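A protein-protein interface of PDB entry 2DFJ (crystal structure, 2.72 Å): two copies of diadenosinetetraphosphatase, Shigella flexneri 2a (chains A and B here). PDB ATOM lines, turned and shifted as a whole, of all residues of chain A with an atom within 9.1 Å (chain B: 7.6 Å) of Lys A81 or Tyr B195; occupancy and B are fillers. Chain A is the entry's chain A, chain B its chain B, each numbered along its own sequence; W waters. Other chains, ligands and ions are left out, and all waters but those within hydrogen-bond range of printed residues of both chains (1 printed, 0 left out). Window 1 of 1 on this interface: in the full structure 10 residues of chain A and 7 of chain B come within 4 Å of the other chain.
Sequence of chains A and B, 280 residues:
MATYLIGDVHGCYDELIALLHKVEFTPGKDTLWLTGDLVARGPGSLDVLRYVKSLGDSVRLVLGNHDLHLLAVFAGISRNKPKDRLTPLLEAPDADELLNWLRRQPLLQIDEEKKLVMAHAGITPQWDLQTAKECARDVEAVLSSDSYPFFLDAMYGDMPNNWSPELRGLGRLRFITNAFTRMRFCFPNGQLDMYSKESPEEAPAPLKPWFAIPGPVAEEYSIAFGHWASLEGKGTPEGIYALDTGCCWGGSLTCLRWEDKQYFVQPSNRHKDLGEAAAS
OD2 of Asp B193 is in hydrogen-bond range of N of Tyr B195.
The side-chain carboxylate (OD2) of Asp B158 is in hydrogen-bond range of the side-chain hydroxyl (OH) of Tyr B195, at 3.2 Å.
Lys A81 touches Tyr B195 (CD to CD1, 3.6 Å).
Phe B187 touches Pro A82 (CZ to CG, 3.8 Å).
O of Pro A82 touches CB of Pro B204 (3.4 Å).
Pro A82 touches Leu B207 (CB to CD1, 3.7 Å).
Lys A83 touches Pro B204.
Pro B204 touches Arg A85.
Val A73 touches none of the printed residues of chain B.
Of the printed residues of chain B, Lys A81 touches Tyr B195 (3.6 Å).
Of the printed residues of chain B, Arg A85 touches Pro B204.
Of the printed residues of chain A, Phe B187 touches Pro A82 (3.8 Å).
Of chain A, only Lys A81 (3.6 Å) comes within 4 Å of Tyr B195.
No residue of chain A comes within 4 Å of Ser B196.
The nearest residue of chain B that does not touch Lys A81 is Asp B193 (5.7 Å).
The nearest residue of chain A that does not touch Tyr B195 is Lys A83 (4.5 Å).
The nearest printed residue of chain B that does not touch Lys A83 is Ser B196 (4.5 Å).
Of the 17 printed residues of chain B, 4 touch a printed residue of chain A.
Hydrophobic or aromatic side chains of chain B that line the printed part of chain A: Phe B187, Tyr B195, Pro B204 and Leu B207.
Among the printed residues, 6 pairs touch across the chains.
Among the printed residues, no Asp or Glu carboxylate lies within 4 Å of a Lys or Arg side-chain nitrogen of the other chain.
No position is printed for both chains.
Water W1 lies within hydrogen-bond range of OD1 of Asp B193 (2.7 Å), OG of Ser B196 (3.1 Å) and N of Lys A83 (3.2 Å).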
ATOM      1  N   VAL A  39      16.128  12.469  10.796  1.00  0.00           N
ATOM      2  CA  VAL A  39      15.599  12.730  12.131  1.00  0.00           C
ATOM      3  C   VAL A  39      16.577  12.794  13.313  1.00  0.00           C
ATOM      4  O   VAL A  39      16.138  12.922  14.457  1.00  0.00           O
ATOM      5  CB  VAL A  39      14.480  11.712  12.485  1.00  0.00           C
ATOM      6  CG1 VAL A  39      13.310  11.842  11.540  1.00  0.00           C
ATOM      7  CG2 VAL A  39      15.021  10.283  12.492  1.00  0.00           C
ATOM      8  N   ALA A  40      17.879  12.716  13.086  1.00  0.00           N
ATOM      9  CA  ALA A  40      18.774  12.619  14.256  1.00  0.00           C
ATOM     10  C   ALA A  40      18.847  13.808  15.239  1.00  0.00           C
ATOM     11  O   ALA A  40      17.909  14.030  15.986  1.00  0.00           O
ATOM     12  CB  ALA A  40      20.170  12.134  13.864  1.00  0.00           C
ATOM     13  N   ARG A  41      19.958  14.540  15.261  1.00  0.00           N
ATOM     14  CA  ARG A  41      20.297  15.350  16.445  1.00  0.00           C
ATOM     15  C   ARG A  41      19.657  16.719  16.493  1.00  0.00           C
ATOM     16  O   ARG A  41      19.368  17.213  17.581  1.00  0.00           O
ATOM     17  CB  ARG A  41      21.817  15.528  16.626  1.00  0.00           C
ATOM     18  CG  ARG A  41      22.697  14.314  16.315  1.00  0.00           C
ATOM     19  CD  ARG A  41      22.435  13.108  17.240  1.00  0.00           C
ATOM     20  NE  ARG A  41      23.316  11.947  16.982  1.00  0.00           N
ATOM     21  CZ  ARG A  41      23.827  11.574  15.792  1.00  0.00           C
ATOM     22  NH1 ARG A  41      23.561  12.247  14.658  1.00  0.00           N
ATOM     23  NH2 ARG A  41      24.613  10.495  15.735  1.00  0.00           N
ATOM     24  N   ASN A  65      20.324   4.715   9.344  1.00  0.00           N
ATOM     25  CA  ASN A  65      20.393   4.095  10.673  1.00  0.00           C
ATOM     26  C   ASN A  65      19.544   4.804  11.732  1.00  0.00           C
ATOM     27  O   ASN A  65      18.858   4.154  12.524  1.00  0.00           O
ATOM     28  CB  ASN A  65      21.848   3.959  11.148  1.00  0.00           C
ATOM     29  CG  ASN A  65      22.659   5.247  10.959  1.00  0.00           C
ATOM     30  OD1 ASN A  65      22.673   5.827   9.871  1.00  0.00           O
ATOM     31  ND2 ASN A  65      23.352   5.687  12.014  1.00  0.00           N
ATOM     32  N   HIS A  66      19.574   6.134  11.737  1.00  0.00           N
ATOM     33  CA  HIS A  66      18.757   6.904  12.682  1.00  0.00           C
ATOM     34  C   HIS A  66      17.259   6.855  12.415  1.00  0.00           C
ATOM     35  O   HIS A  66      16.470   6.934  13.353  1.00  0.00           O
ATOM     36  CB  HIS A  66      19.218   8.349  12.767  1.00  0.00           C
ATOM     37  CG  HIS A  66      20.507   8.520  13.497  1.00  0.00           C
ATOM     38  ND1 HIS A  66      21.735   8.364  12.885  1.00  0.00           N
ATOM     39  CD2 HIS A  66      20.764   8.829  14.790  1.00  0.00           C
ATOM     40  CE1 HIS A  66      22.693   8.578  13.770  1.00  0.00           C
ATOM     41  NE2 HIS A  66      22.131   8.869  14.932  1.00  0.00           N
ATOM     42  N   HIS A  69      16.337   3.665  13.961  1.00  0.00           N
ATOM     43  CA  HIS A  69      16.400   3.815  15.408  1.00  0.00           C
ATOM     44  C   HIS A  69      15.130   4.514  15.893  1.00  0.00           C
ATOM     45  O   HIS A  69      14.494   4.066  16.855  1.00  0.00           O
ATOM     46  CB  HIS A  69      17.647   4.603  15.799  1.00  0.00           C
ATOM     47  CG  HIS A  69      17.752   4.905  17.266  1.00  0.00           C
ATOM     48  ND1 HIS A  69      16.655   5.019  18.094  1.00  0.00           N
ATOM     49  CD2 HIS A  69      18.830   5.168  18.043  1.00  0.00           C
ATOM     50  CE1 HIS A  69      17.052   5.307  19.320  1.00  0.00           C
ATOM     51  NE2 HIS A  69      18.366   5.407  19.316  1.00  0.00           N
ATOM     52  N   LEU A  70      14.762   5.603  15.214  1.00  0.00           N
ATOM     53  CA  LEU A  70      13.513   6.318  15.481  1.00  0.00           C
ATOM     54  C   LEU A  70      12.338   5.355  15.499  1.00  0.00           C
ATOM     55  O   LEU A  70      11.533   5.351  16.444  1.00  0.00           O
ATOM     56  CB  LEU A  70      13.264   7.409  14.438  1.00  0.00           C
ATOM     57  CG  LEU A  70      11.906   8.107  14.571  1.00  0.00           C
ATOM     58  CD1 LEU A  70      11.795   8.910  15.860  1.00  0.00           C
ATOM     59  CD2 LEU A  70      11.654   9.006  13.395  1.00  0.00           C
ATOM     60  N   VAL A  73      12.416   3.158  18.589  1.00  0.00           N
ATOM     61  CA  VAL A  73      11.903   3.856  19.783  1.00  0.00           C
ATOM     62  C   VAL A  73      10.392   3.934  19.765  1.00  0.00           C
ATOM     63  O   VAL A  73       9.740   3.687  20.779  1.00  0.00           O
ATOM     64  CB  VAL A  73      12.440   5.298  19.905  1.00  0.00           C
ATOM     65  CG1 VAL A  73      11.916   5.967  21.160  1.00  0.00           C
ATOM     66  CG2 VAL A  73      13.946   5.312  19.896  1.00  0.00           C
ATOM     67  N   SER A  78      13.522   0.098  21.414  1.00  0.00           N
ATOM     68  CA  SER A  78      14.739   0.676  21.972  1.00  0.00           C
ATOM     69  C   SER A  78      14.412   1.874  22.833  1.00  0.00           C
ATOM     70  O   SER A  78      13.404   2.548  22.610  1.00  0.00           O
ATOM     71  CB  SER A  78      15.703   1.098  20.868  1.00  0.00           C
ATOM     72  OG  SER A  78      15.722   0.155  19.812  1.00  0.00           O
ATOM     73  N   ARG A  79      15.267   2.130  23.821  1.00  0.00           N
ATOM     74  CA  ARG A  79      15.115   3.281  24.715  1.00  0.00           C
ATOM     75  C   ARG A  79      15.427   4.593  23.993  1.00  0.00           C
ATOM     76  O   ARG A  79      16.304   4.651  23.128  1.00  0.00           O
ATOM     77  CB  ARG A  79      16.003   3.121  25.972  1.00  0.00           C
ATOM     78  N   ASN A  80      14.694   5.642  24.352  1.00  0.00           N
ATOM     79  CA  ASN A  80      14.894   6.962  23.768  1.00  0.00           C
ATOM     80  C   ASN A  80      16.101   7.711  24.377  1.00  0.00           C
ATOM     81  O   ASN A  80      16.185   7.897  25.592  1.00  0.00           O
ATOM     82  CB  ASN A  80      13.595   7.785  23.885  1.00  0.00           C
ATOM     83  CG  ASN A  80      13.844   9.273  23.559  1.00  0.00           C
ATOM     84  OD1 ASN A  80      14.927   9.801  23.797  1.00  0.00           O
ATOM     85  ND2 ASN A  80      12.828   9.959  23.041  1.00  0.00           N
ATOM     86  N   LYS A  81      17.009   8.154  23.511  1.00  0.00           N
ATOM     87  CA  LYS A  81      18.164   8.959  23.908  1.00  0.00           C
ATOM     88  C   LYS A  81      17.824  10.450  23.903  1.00  0.00           C
ATOM     89  O   LYS A  81      17.595  11.019  22.827  1.00  0.00           O
ATOM     90  CB  LYS A  81      19.333   8.720  22.941  1.00  0.00           C
ATOM     91  CG  LYS A  81      20.188   7.515  23.270  1.00  0.00           C
ATOM     92  CD  LYS A  81      21.425   7.448  22.372  1.00  0.00           C
ATOM     93  CE  LYS A  81      21.176   6.586  21.133  1.00  0.00           C
ATOM     94  NZ  LYS A  81      22.376   6.608  20.236  1.00  0.00           N
ATOM     95  N   PRO A  82      17.813  11.097  25.092  1.00  0.00           N
ATOM     96  CA  PRO A  82      17.515  12.538  25.161  1.00  0.00           C
ATOM     97  C   PRO A  82      18.249  13.373  24.103  1.00  0.00           C
ATOM     98  O   PRO A  82      17.674  14.315  23.552  1.00  0.00           O
ATOM     99  CB  PRO A  82      17.976  12.923  26.570  1.00  0.00           C
ATOM    100  CG  PRO A  82      17.803  11.676  27.374  1.00  0.00           C
ATOM    101  CD  PRO A  82      18.064  10.523  26.430  1.00  0.00           C
ATOM    102  N   LYS A  83      19.494  13.000  23.809  1.00  0.00           N
ATOM    103  CA  LYS A  83      20.331  13.708  22.833  1.00  0.00           C
ATOM    104  C   LYS A  83      19.752  13.727  21.417  1.00  0.00           C
ATOM    105  O   LYS A  83      20.105  14.593  20.614  1.00  0.00           O
ATOM    106  CB  LYS A  83      21.738  13.106  22.810  1.00  0.00           C
ATOM    107  N   ASP A  84      18.884  12.765  21.118  1.00  0.00           N
ATOM    108  CA  ASP A  84      18.317  12.625  19.784  1.00  0.00           C
ATOM    109  C   ASP A  84      17.229  13.650  19.520  1.00  0.00           C
ATOM    110  O   ASP A  84      16.997  14.018  18.374  1.00  0.00           O
ATOM    111  CB  ASP A  84      17.759  11.218  19.576  1.00  0.00           C
ATOM    112  CG  ASP A  84      18.830  10.207  19.217  1.00  0.00           C
ATOM    113  OD1 ASP A  84      18.637   9.012  19.537  1.00  0.00           O
ATOM    114  OD2 ASP A  84      19.852  10.598  18.609  1.00  0.00           O
ATOM    115  N   ARG A  85      16.563  14.096  20.582  1.00  0.00           N
ATOM    116  CA  ARG A  85      15.551  15.151  20.495  1.00  0.00           C
ATOM    117  C   ARG A  85      14.373  14.765  19.605  1.00  0.00           C
ATOM    118  O   ARG A  85      14.011  15.487  18.678  1.00  0.00           O
ATOM    119  CB  ARG A  85      16.181  16.459  20.018  1.00  0.00           C
ATOM    120  CG  ARG A  85      17.248  16.985  20.943  1.00  0.00           C
ATOM    121  CD  ARG A  85      17.587  18.411  20.608  1.00  0.00           C
ATOM    122  NE  ARG A  85      18.660  18.910  21.466  1.00  0.00           N
ATOM    123  CZ  ARG A  85      18.487  19.386  22.699  1.00  0.00           C
ATOM    124  NH1 ARG A  85      17.268  19.437  23.240  1.00  0.00           N
ATOM    125  NH2 ARG A  85      19.539  19.816  23.393  1.00  0.00           N
ATOM    126  N   LEU A  86      13.784  13.614  19.904  1.00  0.00           N
ATOM    127  CA  LEU A  86      12.707  13.045  19.110  1.00  0.00           C
ATOM    128  C   LEU A  86      11.351  13.211  19.788  1.00  0.00           C
ATOM    129  O   LEU A  86      10.314  12.924  19.176  1.00  0.00           O
ATOM    130  CB  LEU A  86      12.977  11.564  18.846  1.00  0.00           C
ATOM    131  CG  LEU A  86      14.284  11.297  18.109  1.00  0.00           C
ATOM    132  CD1 LEU A  86      14.637   9.814  18.104  1.00  0.00           C
ATOM    133  CD2 LEU A  86      14.214  11.869  16.687  1.00  0.00           C
ATOM    134  N   THR A  87      11.356  13.677  21.042  1.00  0.00           N
ATOM    135  CA  THR A  87      10.115  13.812  21.813  1.00  0.00           C
ATOM    136  C   THR A  87       9.017  14.594  21.070  1.00  0.00           C
ATOM    137  O   THR A  87       7.921  14.064  20.907  1.00  0.00           O
ATOM    138  CB  THR A  87      10.358  14.324  23.268  1.00  0.00           C
ATOM    139  OG1 THR A  87      11.053  13.310  24.003  1.00  0.00           O
ATOM    140  CG2 THR A  87       9.041  14.637  23.997  1.00  0.00           C
ATOM    141  N   LEU A  90       7.709  12.288  18.483  1.00  0.00           N
ATOM    142  CA  LEU A  90       7.023  11.142  19.098  1.00  0.00           C
ATOM    143  C   LEU A  90       5.717  11.552  19.773  1.00  0.00           C
ATOM    144  O   LEU A  90       4.724  10.838  19.668  1.00  0.00           O
ATOM    145  CB  LEU A  90       7.938  10.408  20.094  1.00  0.00           C
ATOM    146  CG  LEU A  90       9.208   9.719  19.564  1.00  0.00           C
ATOM    147  CD1 LEU A  90      10.201   9.439  20.683  1.00  0.00           C
ATOM    148  CD2 LEU A  90       8.899   8.431  18.820  1.00  0.00           C
ATOM    149  N   GLY B 157      30.833  -1.768  27.061  1.00  0.00           N
ATOM    150  CA  GLY B 157      29.403  -1.452  26.935  1.00  0.00           C
ATOM    151  C   GLY B 157      28.860  -0.130  27.485  1.00  0.00           C
ATOM    152  O   GLY B 157      29.605   0.707  28.000  1.00  0.00           O
ATOM    153  N   ASP B 158      27.541   0.042  27.376  1.00  0.00           N
ATOM    154  CA  ASP B 158      26.845   1.237  27.859  1.00  0.00           C
ATOM    155  C   ASP B 158      25.649   0.952  28.765  1.00  0.00           C
ATOM    156  O   ASP B 158      25.165   1.872  29.423  1.00  0.00           O
ATOM    157  CB  ASP B 158      26.334   2.066  26.680  1.00  0.00           C
ATOM    158  CG  ASP B 158      27.429   2.819  25.966  1.00  0.00           C
ATOM    159  OD1 ASP B 158      28.620   2.548  26.205  1.00  0.00           O
ATOM    160  OD2 ASP B 158      27.100   3.694  25.146  1.00  0.00           O
ATOM    161  N   MET B 159      25.178  -0.298  28.818  1.00  0.00           N
ATOM    162  CA  MET B 159      23.759  -0.509  29.144  1.00  0.00           C
ATOM    163  C   MET B 159      23.256  -1.164  30.463  1.00  0.00           C
ATOM    164  O   MET B 159      22.078  -1.596  30.527  1.00  0.00           O
ATOM    165  CB  MET B 159      22.971  -1.037  27.932  1.00  0.00           C
ATOM    166  CG  MET B 159      21.479  -0.689  28.022  1.00  0.00           C
ATOM    167  SD  MET B 159      21.195   0.745  29.127  1.00  0.00           S
ATOM    168  CE  MET B 159      19.505   0.423  29.667  1.00  0.00           C
ATOM    169  N   ASN B 161      22.575   1.022  33.551  1.00  0.00           N
ATOM    170  CA  ASN B 161      22.509   2.451  33.901  1.00  0.00           C
ATOM    171  C   ASN B 161      22.353   2.754  35.377  1.00  0.00           C
ATOM    172  O   ASN B 161      22.688   3.856  35.819  1.00  0.00           O
ATOM    173  CB  ASN B 161      21.326   3.109  33.197  1.00  0.00           C
ATOM    174  CG  ASN B 161      21.671   3.609  31.825  1.00  0.00           C
ATOM    175  OD1 ASN B 161      22.839   3.563  31.399  1.00  0.00           O
ATOM    176  ND2 ASN B 161      20.653   4.094  31.110  1.00  0.00           N
ATOM    177  N   ARG B 182      33.539   7.858  32.658  1.00  0.00           N
ATOM    178  CA  ARG B 182      32.685   8.549  31.690  1.00  0.00           C
ATOM    179  C   ARG B 182      31.297   8.795  32.243  1.00  0.00           C
ATOM    180  O   ARG B 182      30.340   8.107  31.895  1.00  0.00           O
ATOM    181  CB  ARG B 182      32.617   7.814  30.342  1.00  0.00           C
ATOM    182  CG  ARG B 182      32.755   6.305  30.411  1.00  0.00           C
ATOM    183  CD  ARG B 182      32.838   5.715  29.013  1.00  0.00           C
ATOM    184  NE  ARG B 182      31.598   5.044  28.613  1.00  0.00           N
ATOM    185  CZ  ARG B 182      31.149   4.976  27.363  1.00  0.00           C
ATOM    186  NH1 ARG B 182      31.817   5.558  26.372  1.00  0.00           N
ATOM    187  NH2 ARG B 182      30.024   4.333  27.105  1.00  0.00           N
ATOM    188  N   ARG B 184      28.671  12.146  33.049  1.00  0.00           N
ATOM    189  CA  ARG B 184      28.429  13.574  33.039  1.00  0.00           C
ATOM    190  C   ARG B 184      27.040  13.843  33.569  1.00  0.00           C
ATOM    191  O   ARG B 184      26.877  14.361  34.670  1.00  0.00           O
ATOM    192  CB  ARG B 184      28.574  14.142  31.633  1.00  0.00           C
ATOM    193  CG  ARG B 184      29.996  14.367  31.193  1.00  0.00           C
ATOM    194  CD  ARG B 184      30.026  14.867  29.761  1.00  0.00           C
ATOM    195  NE  ARG B 184      31.390  14.972  29.246  1.00  0.00           N
ATOM    196  CZ  ARG B 184      32.116  13.943  28.811  1.00  0.00           C
ATOM    197  NH1 ARG B 184      31.620  12.712  28.825  1.00  0.00           N
ATOM    198  NH2 ARG B 184      33.344  14.153  28.353  1.00  0.00           N
ATOM    199  N   PHE B 185      26.046  13.451  32.780  1.00  0.00           N
ATOM    200  CA  PHE B 185      24.658  13.731  33.078  1.00  0.00           C
ATOM    201  C   PHE B 185      23.948  12.569  33.721  1.00  0.00           C
ATOM    202  O   PHE B 185      24.185  11.413  33.374  1.00  0.00           O
ATOM    203  CB  PHE B 185      23.926  14.096  31.796  1.00  0.00           C
ATOM    204  CG  PHE B 185      24.321  15.418  31.235  1.00  0.00           C
ATOM    205  CD1 PHE B 185      25.238  15.494  30.190  1.00  0.00           C
ATOM    206  CD2 PHE B 185      23.779  16.592  31.748  1.00  0.00           C
ATOM    207  CE1 PHE B 185      25.612  16.728  29.653  1.00  0.00           C
ATOM    208  CE2 PHE B 185      24.141  17.824  31.225  1.00  0.00           C
ATOM    209  CZ  PHE B 185      25.059  17.893  30.170  1.00  0.00           C
ATOM    210  N   PHE B 187      19.856  11.272  34.892  1.00  0.00           N
ATOM    211  CA  PHE B 187      18.420  11.490  34.880  1.00  0.00           C
ATOM    212  C   PHE B 187      18.040  11.994  36.266  1.00  0.00           C
ATOM    213  O   PHE B 187      18.879  11.941  37.155  1.00  0.00           O
ATOM    214  CB  PHE B 187      17.690  10.202  34.503  1.00  0.00           C
ATOM    215  CG  PHE B 187      17.818   9.855  33.045  1.00  0.00           C
ATOM    216  CD1 PHE B 187      18.908   9.119  32.579  1.00  0.00           C
ATOM    217  CD2 PHE B 187      16.864  10.295  32.128  1.00  0.00           C
ATOM    218  CE1 PHE B 187      19.037   8.811  31.224  1.00  0.00           C
ATOM    219  CE2 PHE B 187      16.979   9.990  30.772  1.00  0.00           C
ATOM    220  CZ  PHE B 187      18.066   9.248  30.320  1.00  0.00           C
ATOM    221  N   LEU B 192      22.389   6.977  34.584  1.00  0.00           N
ATOM    222  CA  LEU B 192      23.523   7.487  33.817  1.00  0.00           C
ATOM    223  C   LEU B 192      23.156   7.713  32.366  1.00  0.00           C
ATOM    224  O   LEU B 192      22.621   6.820  31.707  1.00  0.00           O
ATOM    225  CB  LEU B 192      24.719   6.533  33.877  1.00  0.00           C
ATOM    226  CG  LEU B 192      25.596   6.480  35.129  1.00  0.00           C
ATOM    227  CD1 LEU B 192      26.866   5.707  34.832  1.00  0.00           C
ATOM    228  CD2 LEU B 192      25.934   7.866  35.624  1.00  0.00           C
ATOM    229  N   ASP B 193      23.433   8.912  31.874  1.00  0.00           N
ATOM    230  CA  ASP B 193      23.388   9.161  30.450  1.00  0.00           C
ATOM    231  C   ASP B 193      24.796   9.082  29.884  1.00  0.00           C
ATOM    232  O   ASP B 193      25.712   9.731  30.387  1.00  0.00           O
ATOM    233  CB  ASP B 193      22.796  10.525  30.136  1.00  0.00           C
ATOM    234  CG  ASP B 193      22.791  10.807  28.654  1.00  0.00           C
ATOM    235  OD1 ASP B 193      21.829  10.385  27.977  1.00  0.00           O
ATOM    236  OD2 ASP B 193      23.764  11.420  28.158  1.00  0.00           O
ATOM    237  N   MET B 194      24.953   8.305  28.818  1.00  0.00           N
ATOM    238  CA  MET B 194      26.263   8.056  28.237  1.00  0.00           C
ATOM    239  C   MET B 194      26.453   8.723  26.879  1.00  0.00           C
ATOM    240  O   MET B 194      27.336   8.329  26.123  1.00  0.00           O
ATOM    241  CB  MET B 194      26.472   6.548  28.107  1.00  0.00           C
ATOM    242  CG  MET B 194      27.885   6.082  28.404  1.00  0.00           C
ATOM    243  SD  MET B 194      28.428   6.382  30.088  1.00  0.00           S
ATOM    244  CE  MET B 194      27.014   5.776  30.992  1.00  0.00           C
ATOM    245  N   TYR B 195      25.646   9.740  26.576  1.00  0.00           N
ATOM    246  CA  TYR B 195      25.600  10.277  25.210  1.00  0.00           C
ATOM    247  C   TYR B 195      25.741  11.790  25.059  1.00  0.00           C
ATOM    248  O   TYR B 195      26.257  12.252  24.041  1.00  0.00           O
ATOM    249  CB  TYR B 195      24.352   9.773  24.469  1.00  0.00           C
ATOM    250  CG  TYR B 195      24.220   8.267  24.533  1.00  0.00           C
ATOM    251  CD1 TYR B 195      23.335   7.661  25.431  1.00  0.00           C
ATOM    252  CD2 TYR B 195      25.020   7.446  23.736  1.00  0.00           C
ATOM    253  CE1 TYR B 195      23.228   6.277  25.508  1.00  0.00           C
ATOM    254  CE2 TYR B 195      24.926   6.065  23.808  1.00  0.00           C
ATOM    255  CZ  TYR B 195      24.029   5.486  24.695  1.00  0.00           C
ATOM    256  OH  TYR B 195      23.938   4.109  24.762  1.00  0.00           O
ATOM    257  N   SER B 196      25.291  12.567  26.040  1.00  0.00           N
ATOM    258  CA  SER B 196      25.428  14.011  25.906  1.00  0.00           C
ATOM    259  C   SER B 196      26.625  14.582  26.669  1.00  0.00           C
ATOM    260  O   SER B 196      26.890  14.224  27.817  1.00  0.00           O
ATOM    261  CB  SER B 196      24.120  14.740  26.223  1.00  0.00           C
ATOM    262  OG  SER B 196      23.568  14.313  27.445  1.00  0.00           O
ATOM    263  N   LYS B 197      27.354  15.464  25.989  1.00  0.00           N
ATOM    264  CA  LYS B 197      28.574  16.068  26.515  1.00  0.00           C
ATOM    265  C   LYS B 197      28.479  17.556  26.240  1.00  0.00           C
ATOM    266  O   LYS B 197      28.976  18.043  25.231  1.00  0.00           O
ATOM    267  CB  LYS B 197      29.799  15.468  25.814  1.00  0.00           C
ATOM    268  CG  LYS B 197      29.920  13.950  25.930  1.00  0.00           C
ATOM    269  CD  LYS B 197      30.452  13.382  24.534  1.00  0.00           C
ATOM    270  CE  LYS B 197      31.250  12.040  24.979  1.00  0.00           C
ATOM    271  NZ  LYS B 197      31.238  11.151  23.742  1.00  0.00           N
ATOM    272  N   GLU B 198      27.803  18.273  27.124  1.00  0.00           N
ATOM    273  CA  GLU B 198      27.442  19.664  26.872  1.00  0.00           C
ATOM    274  C   GLU B 198      27.405  20.398  28.184  1.00  0.00           C
ATOM    275  O   GLU B 198      27.251  19.785  29.235  1.00  0.00           O
ATOM    276  CB  GLU B 198      26.044  19.760  26.252  1.00  0.00           C
ATOM    277  CG  GLU B 198      25.899  19.233  24.840  1.00  0.00           C
ATOM    278  CD  GLU B 198      24.503  18.673  24.579  1.00  0.00           C
ATOM    279  OE1 GLU B 198      23.753  19.271  23.770  1.00  0.00           O
ATOM    280  OE2 GLU B 198      24.148  17.637  25.187  1.00  0.00           O
ATOM    281  N   PRO B 204      19.624  18.349  26.872  1.00  0.00           N
ATOM    282  CA  PRO B 204      18.205  18.072  26.651  1.00  0.00           C
ATOM    283  C   PRO B 204      17.430  17.771  27.938  1.00  0.00           C
ATOM    284  O   PRO B 204      18.026  17.571  28.991  1.00  0.00           O
ATOM    285  CB  PRO B 204      18.217  16.854  25.717  1.00  0.00           C
ATOM    286  CG  PRO B 204      19.568  16.266  25.853  1.00  0.00           C
ATOM    287  CD  PRO B 204      20.485  17.414  26.126  1.00  0.00           C
ATOM    288  N   LEU B 207      17.838  15.775  31.789  1.00  0.00           N
ATOM    289  CA  LEU B 207      19.208  15.568  32.260  1.00  0.00           C
ATOM    290  C   LEU B 207      19.789  16.689  33.127  1.00  0.00           C
ATOM    291  O   LEU B 207      19.993  17.812  32.666  1.00  0.00           O
ATOM    292  CB  LEU B 207      20.140  15.278  31.078  1.00  0.00           C
ATOM    293  CG  LEU B 207      19.723  14.136  30.147  1.00  0.00           C
ATOM    294  CD1 LEU B 207      20.583  14.121  28.911  1.00  0.00           C
ATOM    295  CD2 LEU B 207      19.779  12.792  30.862  1.00  0.00           C
HETATM  296  O   HOH W   1      21.762  12.243  25.984  1.00  0.00           O
